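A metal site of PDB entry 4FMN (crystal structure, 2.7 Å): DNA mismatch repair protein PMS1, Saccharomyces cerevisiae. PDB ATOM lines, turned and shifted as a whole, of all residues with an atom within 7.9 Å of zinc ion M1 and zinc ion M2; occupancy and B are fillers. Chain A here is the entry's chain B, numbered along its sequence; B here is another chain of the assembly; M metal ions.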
ATOM      1  N   ASP A  68     -11.562  -0.195   2.768  1.00  0.00           N
ATOM      2  CA  ASP A  68     -11.053  -0.528   4.101  1.00  0.00           C
ATOM      3  C   ASP A  68     -10.811  -2.052   4.095  1.00  0.00           C
ATOM      4  O   ASP A  68     -11.779  -2.822   3.950  1.00  0.00           O
ATOM      5  CB  ASP A  68     -12.102  -0.148   5.164  1.00  0.00           C
ATOM      6  CG  ASP A  68     -11.659  -0.273   6.618  1.00  0.00           C
ATOM      7  OD1 ASP A  68     -11.296  -1.418   7.049  1.00  0.00           O
ATOM      8  OD2 ASP A  68     -11.701   0.764   7.352  1.00  0.00           O
ATOM      9  N   HIS A  70     -10.075  -4.260   6.448  1.00  0.00           N
ATOM     10  CA  HIS A  70     -10.756  -5.012   7.510  1.00  0.00           C
ATOM     11  C   HIS A  70     -12.268  -5.104   7.287  1.00  0.00           C
ATOM     12  O   HIS A  70     -12.782  -6.215   7.208  1.00  0.00           O
ATOM     13  CB  HIS A  70     -10.417  -4.481   8.923  1.00  0.00           C
ATOM     14  CG  HIS A  70     -11.206  -5.114  10.017  1.00  0.00           C
ATOM     15  ND1 HIS A  70     -10.942  -6.408  10.451  1.00  0.00           N
ATOM     16  CD2 HIS A  70     -12.269  -4.635  10.722  1.00  0.00           C
ATOM     17  CE1 HIS A  70     -11.839  -6.679  11.397  1.00  0.00           C
ATOM     18  NE2 HIS A  70     -12.660  -5.647  11.590  1.00  0.00           N
ATOM     19  N   ALA A  71     -12.960  -3.961   7.182  1.00  0.00           N
ATOM     20  CA  ALA A  71     -14.423  -3.878   7.034  1.00  0.00           C
ATOM     21  C   ALA A  71     -14.963  -4.604   5.799  1.00  0.00           C
ATOM     22  O   ALA A  71     -15.982  -5.275   5.878  1.00  0.00           O
ATOM     23  CB  ALA A  71     -14.884  -2.422   7.064  1.00  0.00           C
ATOM     24  N   SER A  72     -14.231  -4.541   4.692  1.00  0.00           N
ATOM     25  CA  SER A  72     -14.632  -5.247   3.462  1.00  0.00           C
ATOM     26  C   SER A  72     -14.428  -6.753   3.593  1.00  0.00           C
ATOM     27  O   SER A  72     -15.281  -7.540   3.161  1.00  0.00           O
ATOM     28  CB  SER A  72     -13.878  -4.703   2.259  1.00  0.00           C
ATOM     29  OG  SER A  72     -12.492  -4.833   2.496  1.00  0.00           O
ATOM     30  N   GLU A  74     -14.441  -8.446   6.432  1.00  0.00           N
ATOM     31  CA  GLU A  74     -15.430  -8.739   7.463  1.00  0.00           C
ATOM     32  C   GLU A  74     -16.829  -8.860   6.886  1.00  0.00           C
ATOM     33  O   GLU A  74     -17.506  -9.833   7.211  1.00  0.00           O
ATOM     34  CB  GLU A  74     -15.362  -7.648   8.565  1.00  0.00           C
ATOM     35  CG  GLU A  74     -16.307  -7.894   9.721  1.00  0.00           C
ATOM     36  CD  GLU A  74     -16.245  -6.794  10.742  1.00  0.00           C
ATOM     37  OE1 GLU A  74     -15.197  -6.653  11.411  1.00  0.00           O
ATOM     38  OE2 GLU A  74     -17.241  -6.040  10.841  1.00  0.00           O
ATOM     39  N   LYS A  75     -17.289  -7.886   6.052  1.00  0.00           N
ATOM     40  CA  LYS A  75     -18.644  -7.954   5.461  1.00  0.00           C
ATOM     41  C   LYS A  75     -18.809  -9.257   4.674  1.00  0.00           C
ATOM     42  O   LYS A  75     -19.881  -9.865   4.718  1.00  0.00           O
ATOM     43  CB  LYS A  75     -18.944  -6.713   4.591  1.00  0.00           C
ATOM     44  CG  LYS A  75     -20.327  -6.681   3.898  1.00  0.00           C
ATOM     45  CD  LYS A  75     -21.492  -6.864   4.870  1.00  0.00           C
ATOM     46  CE  LYS A  75     -22.809  -6.382   4.308  1.00  0.00           C
ATOM     47  NZ  LYS A  75     -23.805  -6.142   5.401  1.00  0.00           N
ATOM     48  N   PHE A  78     -18.831 -12.316   7.338  1.00  0.00           N
ATOM     49  CA  PHE A  78     -20.085 -12.166   8.046  1.00  0.00           C
ATOM     50  C   PHE A  78     -21.252 -12.704   7.207  1.00  0.00           C
ATOM     51  O   PHE A  78     -22.020 -13.539   7.702  1.00  0.00           O
ATOM     52  CB  PHE A  78     -20.339 -10.694   8.451  1.00  0.00           C
ATOM     53  CG  PHE A  78     -21.734 -10.406   8.962  1.00  0.00           C
ATOM     54  CD1 PHE A  78     -22.126 -10.798  10.241  1.00  0.00           C
ATOM     55  CD2 PHE A  78     -22.667  -9.753   8.161  1.00  0.00           C
ATOM     56  CE1 PHE A  78     -23.420 -10.555  10.708  1.00  0.00           C
ATOM     57  CE2 PHE A  78     -23.961  -9.510   8.628  1.00  0.00           C
ATOM     58  CZ  PHE A  78     -24.331  -9.909   9.899  1.00  0.00           C
ATOM     59  N   ALA A 180     -21.122 -11.452  13.911  1.00  0.00           N
ATOM     60  CA  ALA A 180     -20.444 -10.172  13.712  1.00  0.00           C
ATOM     61  C   ALA A 180     -19.106 -10.195  14.453  1.00  0.00           C
ATOM     62  O   ALA A 180     -18.122  -9.733  13.916  1.00  0.00           O
ATOM     63  CB  ALA A 180     -21.323  -9.032  14.192  1.00  0.00           C
ATOM     64  N   MET A 181     -19.044 -10.813  15.643  1.00  0.00           N
ATOM     65  CA  MET A 181     -17.792 -10.922  16.377  1.00  0.00           C
ATOM     66  C   MET A 181     -16.881 -11.980  15.763  1.00  0.00           C
ATOM     67  O   MET A 181     -15.678 -11.747  15.679  1.00  0.00           O
ATOM     68  CB  MET A 181     -18.027 -11.188  17.866  1.00  0.00           C
ATOM     69  CG  MET A 181     -16.921 -10.643  18.733  1.00  0.00           C
ATOM     70  SD  MET A 181     -17.301 -10.859  20.491  1.00  0.00           S
ATOM     71  CE  MET A 181     -15.773 -10.220  21.200  1.00  0.00           C
ATOM     72  N   ALA A 183     -16.697 -12.850  12.593  1.00  0.00           N
ATOM     73  CA  ALA A 183     -16.199 -12.209  11.379  1.00  0.00           C
ATOM     74  C   ALA A 183     -15.114 -11.186  11.726  1.00  0.00           C
ATOM     75  O   ALA A 183     -14.043 -11.223  11.127  1.00  0.00           O
ATOM     76  CB  ALA A 183     -17.347 -11.541  10.634  1.00  0.00           C
ATOM     77  N   CYS A 184     -15.363 -10.324  12.706  1.00  0.00           N
ATOM     78  CA  CYS A 184     -14.404  -9.303  13.123  1.00  0.00           C
ATOM     79  C   CYS A 184     -13.052  -9.872  13.593  1.00  0.00           C
ATOM     80  O   CYS A 184     -11.998  -9.325  13.259  1.00  0.00           O
ATOM     81  CB  CYS A 184     -15.023  -8.384  14.170  1.00  0.00           C
ATOM     82  SG  CYS A 184     -13.952  -7.026  14.677  1.00  0.00           S
ATOM     83  N   ARG A 185     -13.083 -10.977  14.336  1.00  0.00           N
ATOM     84  CA  ARG A 185     -11.899 -11.632  14.862  1.00  0.00           C
ATOM     85  C   ARG A 185     -11.137 -12.450  13.816  1.00  0.00           C
ATOM     86  O   ARG A 185      -9.930 -12.583  13.911  1.00  0.00           O
ATOM     87  CB  ARG A 185     -12.249 -12.481  16.107  1.00  0.00           C
ATOM     88  CG  ARG A 185     -12.796 -11.641  17.259  1.00  0.00           C
ATOM     89  CD  ARG A 185     -12.805 -12.368  18.592  1.00  0.00           C
ATOM     90  NE  ARG A 185     -11.567 -12.128  19.349  1.00  0.00           N
ATOM     91  CZ  ARG A 185     -11.492 -11.386  20.450  1.00  0.00           C
ATOM     92  NH1 ARG A 185     -12.572 -10.809  20.948  1.00  0.00           N
ATOM     93  NH2 ARG A 185     -10.320 -11.229  21.066  1.00  0.00           N
ATOM     94  N   SER A 186     -11.825 -13.006  12.817  1.00  0.00           N
ATOM     95  CA  SER A 186     -11.184 -13.835  11.814  1.00  0.00           C
ATOM     96  C   SER A 186     -10.736 -13.094  10.538  1.00  0.00           C
ATOM     97  O   SER A 186      -9.954 -13.623   9.759  1.00  0.00           O
ATOM     98  CB  SER A 186     -12.090 -15.011  11.455  1.00  0.00           C
ATOM     99  OG  SER A 186     -13.211 -14.603  10.690  1.00  0.00           O
ATOM    100  N   SER A 187     -11.247 -11.865  10.333  1.00  0.00           N
ATOM    101  CA  SER A 187     -10.939 -11.058   9.170  1.00  0.00           C
ATOM    102  C   SER A 187      -9.538 -10.425   9.206  1.00  0.00           C
ATOM    103  O   SER A 187      -8.849 -10.473  10.233  1.00  0.00           O
ATOM    104  CB  SER A 187     -12.011  -9.995   8.985  1.00  0.00           C
ATOM    105  OG  SER A 187     -13.243 -10.648   8.728  1.00  0.00           O
ATOM    106  N   ILE A 188      -9.116  -9.867   8.062  1.00  0.00           N
ATOM    107  CA  ILE A 188      -7.825  -9.200   7.883  1.00  0.00           C
ATOM    108  C   ILE A 188      -7.779  -8.027   8.854  1.00  0.00           C
ATOM    109  O   ILE A 188      -8.746  -7.255   8.938  1.00  0.00           O
ATOM    110  CB  ILE A 188      -7.615  -8.762   6.391  1.00  0.00           C
ATOM    111  CG1 ILE A 188      -7.238  -9.958   5.547  1.00  0.00           C
ATOM    112  CG2 ILE A 188      -6.578  -7.617   6.188  1.00  0.00           C
ATOM    113  CD1 ILE A 188      -7.663  -9.824   4.142  1.00  0.00           C
ATOM    114  N   ASN A 214     -21.426  -1.427   3.978  1.00  0.00           N
ATOM    115  CA  ASN A 214     -21.096  -1.398   5.398  1.00  0.00           C
ATOM    116  C   ASN A 214     -20.808  -2.750   5.965  1.00  0.00           C
ATOM    117  O   ASN A 214     -21.390  -3.730   5.511  1.00  0.00           O
ATOM    118  CB  ASN A 214     -22.225  -0.760   6.232  1.00  0.00           C
ATOM    119  CG  ASN A 214     -22.473   0.676   5.891  1.00  0.00           C
ATOM    120  OD1 ASN A 214     -21.644   1.552   6.134  1.00  0.00           O
ATOM    121  ND2 ASN A 214     -23.639   0.924   5.300  1.00  0.00           N
ATOM    122  N   CYS A 215     -19.968  -2.799   7.015  1.00  0.00           N
ATOM    123  CA  CYS A 215     -19.632  -4.012   7.745  1.00  0.00           C
ATOM    124  C   CYS A 215     -20.826  -4.275   8.700  1.00  0.00           C
ATOM    125  O   CYS A 215     -21.657  -3.369   8.895  1.00  0.00           O
ATOM    126  CB  CYS A 215     -18.328  -3.791   8.518  1.00  0.00           C
ATOM    127  SG  CYS A 215     -18.548  -3.071  10.174  1.00  0.00           S
ATOM    128  N   PRO A 216     -20.901  -5.439   9.383  1.00  0.00           N
ATOM    129  CA  PRO A 216     -22.031  -5.662  10.324  1.00  0.00           C
ATOM    130  C   PRO A 216     -22.167  -4.661  11.492  1.00  0.00           C
ATOM    131  O   PRO A 216     -23.225  -4.586  12.105  1.00  0.00           O
ATOM    132  CB  PRO A 216     -21.825  -7.085  10.811  1.00  0.00           C
ATOM    133  CG  PRO A 216     -20.393  -7.397  10.515  1.00  0.00           C
ATOM    134  CD  PRO A 216     -20.043  -6.639   9.294  1.00  0.00           C
ATOM    135  N   HIS A 217     -21.108  -3.886  11.795  1.00  0.00           N
ATOM    136  CA  HIS A 217     -21.163  -2.893  12.870  1.00  0.00           C
ATOM    137  C   HIS A 217     -21.588  -1.517  12.346  1.00  0.00           C
ATOM    138  O   HIS A 217     -21.763  -0.603  13.143  1.00  0.00           O
ATOM    139  CB  HIS A 217     -19.825  -2.806  13.597  1.00  0.00           C
ATOM    140  CG  HIS A 217     -19.314  -4.130  14.002  1.00  0.00           C
ATOM    141  ND1 HIS A 217     -18.461  -4.835  13.169  1.00  0.00           N
ATOM    142  CD2 HIS A 217     -19.604  -4.878  15.096  1.00  0.00           C
ATOM    143  CE1 HIS A 217     -18.232  -5.983  13.798  1.00  0.00           C
ATOM    144  NE2 HIS A 217     -18.888  -6.028  14.979  1.00  0.00           N
ATOM    145  N   GLY A 218     -21.743  -1.387  11.030  1.00  0.00           N
ATOM    146  CA  GLY A 218     -22.174  -0.150  10.382  1.00  0.00           C
ATOM    147  C   GLY A 218     -21.080   0.757   9.860  1.00  0.00           C
ATOM    148  O   GLY A 218     -21.351   1.912   9.517  1.00  0.00           O
ATOM    149  N   ARG A 219     -19.836   0.258   9.812  1.00  0.00           N
ATOM    150  CA  ARG A 219     -18.667   1.011   9.344  1.00  0.00           C
ATOM    151  C   ARG A 219     -18.545   0.860   7.831  1.00  0.00           C
ATOM    152  O   ARG A 219     -18.817  -0.213   7.316  1.00  0.00           O
ATOM    153  CB  ARG A 219     -17.376   0.496  10.010  1.00  0.00           C
ATOM    154  CG  ARG A 219     -17.432   0.353  11.501  1.00  0.00           C
ATOM    155  CD  ARG A 219     -17.719   1.654  12.208  1.00  0.00           C
ATOM    156  NE  ARG A 219     -18.358   1.384  13.493  1.00  0.00           N
ATOM    157  CZ  ARG A 219     -19.030   2.267  14.202  1.00  0.00           C
ATOM    158  NH1 ARG A 219     -19.155   3.513  13.772  1.00  0.00           N
ATOM    159  NH2 ARG A 219     -19.608   1.904  15.341  1.00  0.00           N
ATOM    160  N   PRO A 220     -18.098   1.898   7.106  1.00  0.00           N
ATOM    161  CA  PRO A 220     -18.030   1.767   5.642  1.00  0.00           C
ATOM    162  C   PRO A 220     -16.932   0.833   5.176  1.00  0.00           C
ATOM    163  O   PRO A 220     -15.879   0.744   5.809  1.00  0.00           O
ATOM    164  CB  PRO A 220     -17.862   3.212   5.154  1.00  0.00           C
ATOM    165  CG  PRO A 220     -17.328   3.934   6.266  1.00  0.00           C
ATOM    166  CD  PRO A 220     -17.751   3.267   7.531  1.00  0.00           C
ATOM    167  N   GLU B 286     -14.089   3.882  10.240  1.00  0.00           N
ATOM    168  CA  GLU B 286     -13.899   3.767  11.698  1.00  0.00           C
ATOM    169  C   GLU B 286     -13.839   2.322  12.164  1.00  0.00           C
ATOM    170  O   GLU B 286     -14.385   1.440  11.502  1.00  0.00           O
ATOM    171  CB  GLU B 286     -15.005   4.512  12.478  1.00  0.00           C
ATOM    172  CG  GLU B 286     -15.430   5.879  11.949  1.00  0.00           C
ATOM    173  CD  GLU B 286     -16.229   6.724  12.923  1.00  0.00           C
ATOM    174  OE1 GLU B 286     -17.258   6.233  13.451  1.00  0.00           O
ATOM    175  OE2 GLU B 286     -15.810   7.882  13.170  1.00  0.00           O
ATOM    176  N   ARG B 287     -13.221   2.088  13.329  1.00  0.00           N
ATOM    177  CA  ARG B 287     -13.107   0.782  13.938  1.00  0.00           C
ATOM    178  C   ARG B 287     -14.503   0.232  14.282  1.00  0.00           C
ATOM    179  O   ARG B 287     -15.426   0.989  14.565  1.00  0.00           O
ATOM    180  CB  ARG B 287     -12.226   0.823  15.181  1.00  0.00           C
ATOM    181  CG  ARG B 287     -12.831   1.584  16.377  1.00  0.00           C
ATOM    182  CD  ARG B 287     -11.821   1.917  17.454  1.00  0.00           C
ATOM    183  NE  ARG B 287     -10.711   2.713  16.927  1.00  0.00           N
ATOM    184  CZ  ARG B 287      -9.637   3.034  17.640  1.00  0.00           C
ATOM    185  NH1 ARG B 287      -9.530   2.645  18.909  1.00  0.00           N
ATOM    186  NH2 ARG B 287      -8.651   3.731  17.085  1.00  0.00           N
ATOM    187  N   CYS B 288     -14.617  -1.107  14.224  1.00  0.00           N
ATOM    188  CA  CYS B 288     -15.845  -1.819  14.488  1.00  0.00           C
ATOM    189  C   CYS B 288     -16.169  -1.617  15.926  1.00  0.00           C
ATOM    190  O   CYS B 288     -15.243  -1.853  16.731  1.00  0.00           O
ATOM    191  CB  CYS B 288     -15.684  -3.298  14.139  1.00  0.00           C
ATOM    192  SG  CYS B 288     -15.230  -3.602  12.422  1.00  0.00           S
ATOM    193  OXT CYS B 288     -17.226  -1.038  16.208  1.00  0.00           O
HETATM  194 ZN    ZN M   1     -14.334  -5.649  12.737  1.00  0.00          ZN
HETATM  195 ZN    ZN M   2     -17.299  -4.310  11.720  1.00  0.00          ZN
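OG of Ser 187 lies close to N of Glu 74 (3.4 Å).
A ring nitrogen (ND1) of His 70 is in hydrogen-bond range of the backbone carbonyl oxygen (O) of Ile 188.
The backbone NH (N) of His 70 lies within hydrogen-bond range of the side-chain carboxylate (OD1) of Asp 68, 3.2 Å away.
The chain-end carboxylate of Cys 288 of chain B lies within salt-bridge range of the guanidinium group of Arg 219.
SG of Cys 215 lies close to N of Arg 219, at 3.6 Å.
The side-chain sulfur (SG) of Cys 215 lies close to the backbone NH (N) of Gly 218 (3.7 Å).
The nearest printed residue that does not touch zinc ion M1 is His 217 (4.1 Å).
Four residues have an atom within 4 Å of zinc ion M2: Glu 74, Cys 215, His 217 and Cys 288 of chain B.
OE1 of Glu 74 is bound to zinc ion M1, at 1.9 Å.
A ring nitrogen (NE2) of His 70 binds zinc ion M1 (2.0 Å).
Zinc ion M1 is bound by SG of Cys 288 of chain B (2.3 Å).
SG of Cys 184 binds zinc ion M1 (2.4 Å).
ND1 of His 217 binds zinc ion M2, 1.9 Å away.
Zinc ion M2 is bound by OE2 of Glu 74, 1.9 Å away.
Zinc ion M2 is bound by the side-chain sulfur (SG) of Cys 288 of chain B (2.3 Å).
SG of Cys 215 is bound to zinc ion M2.
Zinc ion M2 has four donor atoms within binding distance.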
